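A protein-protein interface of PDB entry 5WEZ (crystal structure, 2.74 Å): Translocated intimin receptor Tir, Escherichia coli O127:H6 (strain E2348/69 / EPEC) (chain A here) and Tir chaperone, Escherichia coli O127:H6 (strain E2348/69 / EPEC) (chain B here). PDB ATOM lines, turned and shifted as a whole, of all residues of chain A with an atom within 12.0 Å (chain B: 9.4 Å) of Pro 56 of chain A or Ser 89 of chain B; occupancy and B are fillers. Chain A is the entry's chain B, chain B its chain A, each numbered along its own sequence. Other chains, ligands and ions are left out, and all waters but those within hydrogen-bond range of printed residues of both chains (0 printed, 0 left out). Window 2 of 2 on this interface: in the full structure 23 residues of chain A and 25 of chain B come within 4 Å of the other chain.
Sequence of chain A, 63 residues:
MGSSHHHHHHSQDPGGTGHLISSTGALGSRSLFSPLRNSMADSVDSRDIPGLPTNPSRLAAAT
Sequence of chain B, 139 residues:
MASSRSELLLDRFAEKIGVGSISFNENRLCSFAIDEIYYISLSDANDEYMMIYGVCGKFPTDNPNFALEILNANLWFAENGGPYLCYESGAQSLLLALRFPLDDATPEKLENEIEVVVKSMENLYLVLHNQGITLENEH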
ATOM      1  N   PRO A  50     -13.234  22.916 -11.985  1.00  0.00           N
ATOM      2  CA  PRO A  50     -14.171  22.025 -12.676  1.00  0.00           C
ATOM      3  C   PRO A  50     -14.469  22.176 -14.179  1.00  0.00           C
ATOM      4  O   PRO A  50     -14.585  21.129 -14.803  1.00  0.00           O
ATOM      5  CB  PRO A  50     -15.431  22.167 -11.830  1.00  0.00           C
ATOM      6  CG  PRO A  50     -14.875  22.288 -10.440  1.00  0.00           C
ATOM      7  CD  PRO A  50     -13.511  22.940 -10.540  1.00  0.00           C
ATOM      8  N   GLY A  51     -14.588  23.364 -14.758  1.00  0.00           N
ATOM      9  CA  GLY A  51     -14.870  23.433 -16.187  1.00  0.00           C
ATOM     10  C   GLY A  51     -16.123  22.660 -16.534  1.00  0.00           C
ATOM     11  O   GLY A  51     -16.157  21.844 -17.439  1.00  0.00           O
ATOM     12  N   LEU A  52     -17.170  22.967 -15.795  1.00  0.00           N
ATOM     13  CA  LEU A  52     -18.470  22.333 -15.878  1.00  0.00           C
ATOM     14  C   LEU A  52     -19.150  22.427 -17.217  1.00  0.00           C
ATOM     15  O   LEU A  52     -18.893  23.332 -17.986  1.00  0.00           O
ATOM     16  CB  LEU A  52     -19.386  23.078 -14.927  1.00  0.00           C
ATOM     17  CG  LEU A  52     -19.355  24.572 -15.271  1.00  0.00           C
ATOM     18  CD1 LEU A  52     -20.338  24.930 -16.359  1.00  0.00           C
ATOM     19  CD2 LEU A  52     -19.591  25.450 -14.062  1.00  0.00           C
ATOM     20  N   PRO A  53     -20.030  21.397 -17.502  1.00  0.00           N
ATOM     21  CA  PRO A  53     -20.725  21.511 -18.775  1.00  0.00           C
ATOM     22  C   PRO A  53     -22.172  21.897 -18.511  1.00  0.00           C
ATOM     23  O   PRO A  53     -22.955  21.956 -19.447  1.00  0.00           O
ATOM     24  CB  PRO A  53     -20.706  20.093 -19.281  1.00  0.00           C
ATOM     25  CG  PRO A  53     -21.049  19.312 -18.059  1.00  0.00           C
ATOM     26  CD  PRO A  53     -20.558  20.111 -16.869  1.00  0.00           C
ATOM     27  N   THR A  54     -22.539  22.134 -17.257  1.00  0.00           N
ATOM     28  CA  THR A  54     -23.913  22.547 -16.982  1.00  0.00           C
ATOM     29  C   THR A  54     -24.076  22.879 -15.508  1.00  0.00           C
ATOM     30  O   THR A  54     -23.458  22.260 -14.640  1.00  0.00           O
ATOM     31  CB  THR A  54     -24.928  21.476 -17.393  1.00  0.00           C
ATOM     32  OG1 THR A  54     -24.966  21.388 -18.821  1.00  0.00           O
ATOM     33  CG2 THR A  54     -26.321  21.821 -16.908  1.00  0.00           C
ATOM     34  N   ASN A  55     -24.908  23.887 -15.250  1.00  0.00           N
ATOM     35  CA  ASN A  55     -25.350  24.441 -13.981  1.00  0.00           C
ATOM     36  C   ASN A  55     -26.865  24.284 -13.856  1.00  0.00           C
ATOM     37  O   ASN A  55     -27.564  24.216 -14.872  1.00  0.00           O
ATOM     38  CB  ASN A  55     -24.976  25.928 -13.882  1.00  0.00           C
ATOM     39  CG  ASN A  55     -24.070  26.396 -15.027  1.00  0.00           C
ATOM     40  OD1 ASN A  55     -23.817  25.661 -15.982  1.00  0.00           O
ATOM     41  ND2 ASN A  55     -23.591  27.636 -14.934  1.00  0.00           N
ATOM     42  N   PRO A  56     -27.407  24.225 -12.638  1.00  0.00           N
ATOM     43  CA  PRO A  56     -28.837  23.923 -12.474  1.00  0.00           C
ATOM     44  C   PRO A  56     -29.720  25.135 -12.732  1.00  0.00           C
ATOM     45  O   PRO A  56     -29.666  26.134 -12.006  1.00  0.00           O
ATOM     46  CB  PRO A  56     -28.923  23.451 -11.016  1.00  0.00           C
ATOM     47  CG  PRO A  56     -27.836  24.200 -10.332  1.00  0.00           C
ATOM     48  CD  PRO A  56     -26.718  24.326 -11.338  1.00  0.00           C
ATOM     49  N   SER A  57     -30.535  25.052 -13.789  1.00  0.00           N
ATOM     50  CA  SER A  57     -31.634  25.998 -13.962  1.00  0.00           C
ATOM     51  C   SER A  57     -32.710  25.772 -12.909  1.00  0.00           C
ATOM     52  O   SER A  57     -33.322  26.728 -12.413  1.00  0.00           O
ATOM     53  CB  SER A  57     -32.240  25.864 -15.366  1.00  0.00           C
ATOM     54  OG  SER A  57     -33.083  24.723 -15.474  1.00  0.00           O
ATOM     55  N   ARG A  58     -32.939  24.511 -12.554  1.00  0.00           N
ATOM     56  CA  ARG A  58     -34.019  24.128 -11.670  1.00  0.00           C
ATOM     57  C   ARG A  58     -33.957  22.634 -11.352  1.00  0.00           C
ATOM     58  O   ARG A  58     -33.109  21.908 -11.872  1.00  0.00           O
ATOM     59  CB  ARG A  58     -35.360  24.479 -12.307  1.00  0.00           C
ATOM     60  N   TYR B  53     -18.515  32.488 -18.385  1.00  0.00           N
ATOM     61  CA  TYR B  53     -18.230  31.946 -17.073  1.00  0.00           C
ATOM     62  C   TYR B  53     -16.728  31.860 -16.856  1.00  0.00           C
ATOM     63  O   TYR B  53     -15.999  31.344 -17.710  1.00  0.00           O
ATOM     64  CB  TYR B  53     -18.878  30.592 -16.943  1.00  0.00           C
ATOM     65  CG  TYR B  53     -20.370  30.706 -16.977  1.00  0.00           C
ATOM     66  CD1 TYR B  53     -21.050  31.421 -16.000  1.00  0.00           C
ATOM     67  CD2 TYR B  53     -21.109  30.101 -17.973  1.00  0.00           C
ATOM     68  CE1 TYR B  53     -22.423  31.517 -15.998  1.00  0.00           C
ATOM     69  CE2 TYR B  53     -22.485  30.199 -17.983  1.00  0.00           C
ATOM     70  CZ  TYR B  53     -23.135  30.906 -16.994  1.00  0.00           C
ATOM     71  OH  TYR B  53     -24.510  31.009 -17.010  1.00  0.00           O
ATOM     72  N   PHE B  59     -14.866  25.411  -4.008  1.00  0.00           N
ATOM     73  CA  PHE B  59     -15.167  26.510  -3.099  1.00  0.00           C
ATOM     74  C   PHE B  59     -14.886  26.073  -1.671  1.00  0.00           C
ATOM     75  O   PHE B  59     -15.524  25.128  -1.184  1.00  0.00           O
ATOM     76  CB  PHE B  59     -16.626  26.939  -3.259  1.00  0.00           C
ATOM     77  CG  PHE B  59     -17.008  28.164  -2.471  1.00  0.00           C
ATOM     78  CD1 PHE B  59     -17.268  28.078  -1.110  1.00  0.00           C
ATOM     79  CD2 PHE B  59     -17.159  29.392  -3.099  1.00  0.00           C
ATOM     80  CE1 PHE B  59     -17.630  29.193  -0.387  1.00  0.00           C
ATOM     81  CE2 PHE B  59     -17.528  30.514  -2.382  1.00  0.00           C
ATOM     82  CZ  PHE B  59     -17.764  30.413  -1.022  1.00  0.00           C
ATOM     83  N   CYS B  86     -20.550  34.513  -8.231  1.00  0.00           N
ATOM     84  CA  CYS B  86     -21.625  33.567  -7.965  1.00  0.00           C
ATOM     85  C   CYS B  86     -21.085  32.227  -7.502  1.00  0.00           C
ATOM     86  O   CYS B  86     -19.998  31.807  -7.906  1.00  0.00           O
ATOM     87  CB  CYS B  86     -22.446  33.309  -9.195  1.00  0.00           C
ATOM     88  SG  CYS B  86     -22.863  34.816  -9.999  1.00  0.00           S
ATOM     89  N   TYR B  87     -21.879  31.530  -6.690  1.00  0.00           N
ATOM     90  CA  TYR B  87     -21.572  30.164  -6.280  1.00  0.00           C
ATOM     91  C   TYR B  87     -22.461  29.171  -7.017  1.00  0.00           C
ATOM     92  O   TYR B  87     -23.674  29.371  -7.133  1.00  0.00           O
ATOM     93  CB  TYR B  87     -21.744  29.968  -4.777  1.00  0.00           C
ATOM     94  CG  TYR B  87     -21.627  28.512  -4.388  1.00  0.00           C
ATOM     95  CD1 TYR B  87     -20.394  27.948  -4.107  1.00  0.00           C
ATOM     96  CD2 TYR B  87     -22.748  27.695  -4.325  1.00  0.00           C
ATOM     97  CE1 TYR B  87     -20.281  26.622  -3.769  1.00  0.00           C
ATOM     98  CE2 TYR B  87     -22.649  26.378  -3.992  1.00  0.00           C
ATOM     99  CZ  TYR B  87     -21.413  25.840  -3.712  1.00  0.00           C
ATOM    100  OH  TYR B  87     -21.314  24.507  -3.370  1.00  0.00           O
ATOM    101  N   GLU B  88     -21.855  28.083  -7.477  1.00  0.00           N
ATOM    102  CA  GLU B  88     -22.531  27.056  -8.253  1.00  0.00           C
ATOM    103  C   GLU B  88     -22.481  25.744  -7.484  1.00  0.00           C
ATOM    104  O   GLU B  88     -21.450  25.400  -6.900  1.00  0.00           O
ATOM    105  CB  GLU B  88     -21.872  26.904  -9.631  1.00  0.00           C
ATOM    106  CG  GLU B  88     -22.752  26.301 -10.718  1.00  0.00           C
ATOM    107  CD  GLU B  88     -22.727  24.787 -10.734  1.00  0.00           C
ATOM    108  OE1 GLU B  88     -23.742  24.196 -10.317  1.00  0.00           O
ATOM    109  OE2 GLU B  88     -21.697  24.193 -11.143  1.00  0.00           O
ATOM    110  N   SER B  89     -23.596  25.003  -7.499  1.00  0.00           N
ATOM    111  CA  SER B  89     -23.771  23.847  -6.624  1.00  0.00           C
ATOM    112  C   SER B  89     -23.365  22.515  -7.247  1.00  0.00           C
ATOM    113  O   SER B  89     -23.062  21.573  -6.505  1.00  0.00           O
ATOM    114  CB  SER B  89     -25.230  23.765  -6.172  1.00  0.00           C
ATOM    115  OG  SER B  89     -26.107  24.006  -7.261  1.00  0.00           O
ATOM    116  N   GLY B  90     -23.350  22.407  -8.577  1.00  0.00           N
ATOM    117  CA  GLY B  90     -23.081  21.123  -9.205  1.00  0.00           C
ATOM    118  C   GLY B  90     -21.622  20.718  -9.147  1.00  0.00           C
ATOM    119  O   GLY B  90     -21.300  19.525  -9.147  1.00  0.00           O
ATOM    120  N   ALA B  91     -20.721  21.696  -9.113  1.00  0.00           N
ATOM    121  CA  ALA B  91     -19.297  21.453  -8.952  1.00  0.00           C
ATOM    122  C   ALA B  91     -18.762  22.101  -7.686  1.00  0.00           C
ATOM    123  O   ALA B  91     -17.542  22.120  -7.480  1.00  0.00           O
ATOM    124  CB  ALA B  91     -18.526  21.969 -10.170  1.00  0.00           C
ATOM    125  N   GLN B  92     -19.647  22.640  -6.843  1.00  0.00           N
ATOM    126  CA  GLN B  92     -19.264  23.395  -5.647  1.00  0.00           C
ATOM    127  C   GLN B  92     -18.224  24.463  -5.975  1.00  0.00           C
ATOM    128  O   GLN B  92     -17.432  24.855  -5.123  1.00  0.00           O
ATOM    129  CB  GLN B  92     -18.758  22.466  -4.536  1.00  0.00           C
ATOM    130  N   SER B  93     -18.223  24.945  -7.217  1.00  0.00           N
ATOM    131  CA  SER B  93     -17.165  25.812  -7.723  1.00  0.00           C
ATOM    132  C   SER B  93     -17.587  27.270  -7.679  1.00  0.00           C
ATOM    133  O   SER B  93     -18.759  27.592  -7.873  1.00  0.00           O
ATOM    134  CB  SER B  93     -16.773  25.433  -9.156  1.00  0.00           C
ATOM    135  OG  SER B  93     -17.904  25.098  -9.942  1.00  0.00           O
ATOM    136  N   LEU B  94     -16.626  28.146  -7.406  1.00  0.00           N
ATOM    137  CA  LEU B  94     -16.861  29.570  -7.562  1.00  0.00           C
ATOM    138  C   LEU B  94     -16.964  29.901  -9.052  1.00  0.00           C
ATOM    139  O   LEU B  94     -16.605  29.098  -9.919  1.00  0.00           O
ATOM    140  CB  LEU B  94     -15.751  30.370  -6.875  1.00  0.00           C
ATOM    141  CG  LEU B  94     -15.816  31.887  -6.720  1.00  0.00           C
ATOM    142  CD1 LEU B  94     -14.974  32.312  -5.612  1.00  0.00           C
ATOM    143  CD2 LEU B  94     -15.270  32.548  -7.928  1.00  0.00           C
ATOM    144  N   LEU B  95     -17.504  31.078  -9.344  1.00  0.00           N
ATOM    145  CA  LEU B  95     -17.745  31.485 -10.722  1.00  0.00           C
ATOM    146  C   LEU B  95     -17.797  33.003 -10.816  1.00  0.00           C
ATOM    147  O   LEU B  95     -18.445  33.656  -9.992  1.00  0.00           O
ATOM    148  CB  LEU B  95     -19.069  30.900 -11.245  1.00  0.00           C
ATOM    149  CG  LEU B  95     -19.147  29.521 -11.890  1.00  0.00           C
ATOM    150  CD1 LEU B  95     -20.396  29.485 -12.789  1.00  0.00           C
ATOM    151  CD2 LEU B  95     -17.840  29.169 -12.655  1.00  0.00           C
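Among the printed residues, pairs that only touch across the chains: Pro 56 of chain A with Glu 88 of chain B, Pro 50 of chain A with Ala 91 of chain B, Pro 56 of chain A with Ser 89 of chain B, Leu 52 of chain A with Glu 88 of chain B, Asn 55 of chain A with Glu 88 of chain B, Pro 50 of chain A with Ser 93 of chain B and Asn 55 of chain A with Tyr 53 of chain B.
Printed residues of chain A that touch a printed residue of chain B: Pro 50, Leu 52, Asn 55 and Pro 56. Hydrophobic or aromatic side chains of chain A within 4 Å of the printed part of chain B: Pro 50, Leu 52 and Pro 56. Hydrophobic or aromatic side chains of chain B within 4 Å of the printed part of chain A: Tyr 53 and Ala 91. Along chain B the printed residues that touch a printed residue of chain A span positions 53 to 93. Among the printed residues, 7 pairs touch across the chains. Among the printed residues, no Asp or Glu carboxylate lies within 4 Å of a Lys or Arg side-chain nitrogen of the other chain.
OE1 of Glu 88 of chain B lies within hydrogen-bond range of N of Gly 90 of chain B (2.5 Å). OE2 of Glu 88 of chain B lies within hydrogen-bond range of N of Ala 91 of chain B (3.4 Å). N of Glu 88 of chain B is in hydrogen-bond range of O of Ser 93 of chain B (3.2 Å).
Of the printed residues of chain B, Pro 56 of chain A touches Glu 88 (3.1 Å) and Ser 89 (3.5 Å). Of chain A, only Pro 56 (3.5 Å) comes within 4 Å of Ser 89 of chain B. No residue of chain B comes within 4 Å of Ser 57 of chain A. No residue of chain A comes within 4 Å of Tyr 87 of chain B. Glu 88 of chain B touches just these residues of chain A: Leu 52, Asn 55 and Pro 56. Of chain A, only Pro 50 (3.5 Å) comes within 4 Å of Ala 91 of chain B. No residue of chain A comes within 4 Å of Gln 92 of chain B. Of the printed residues of chain B, Pro 50 of chain A touches Ala 91 (3.5 Å) and Ser 93 (3.9 Å). Printed residues of chain B within 4 Å of Leu 52 of chain A: Glu 88 (3.8 Å). Of the printed residues of chain B, Asn 55 of chain A touches Tyr 53 and Glu 88. Printed residues of chain A within 4 Å of Tyr 53 of chain B: Asn 55 (3.9 Å). The nearest residue of chain B that does not touch Pro 56 of chain A is Gly 90 of chain B (4.8 Å). The nearest printed residue of chain B that does not touch Asn 55 of chain A is Leu 95 of chain B (4.3 Å).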
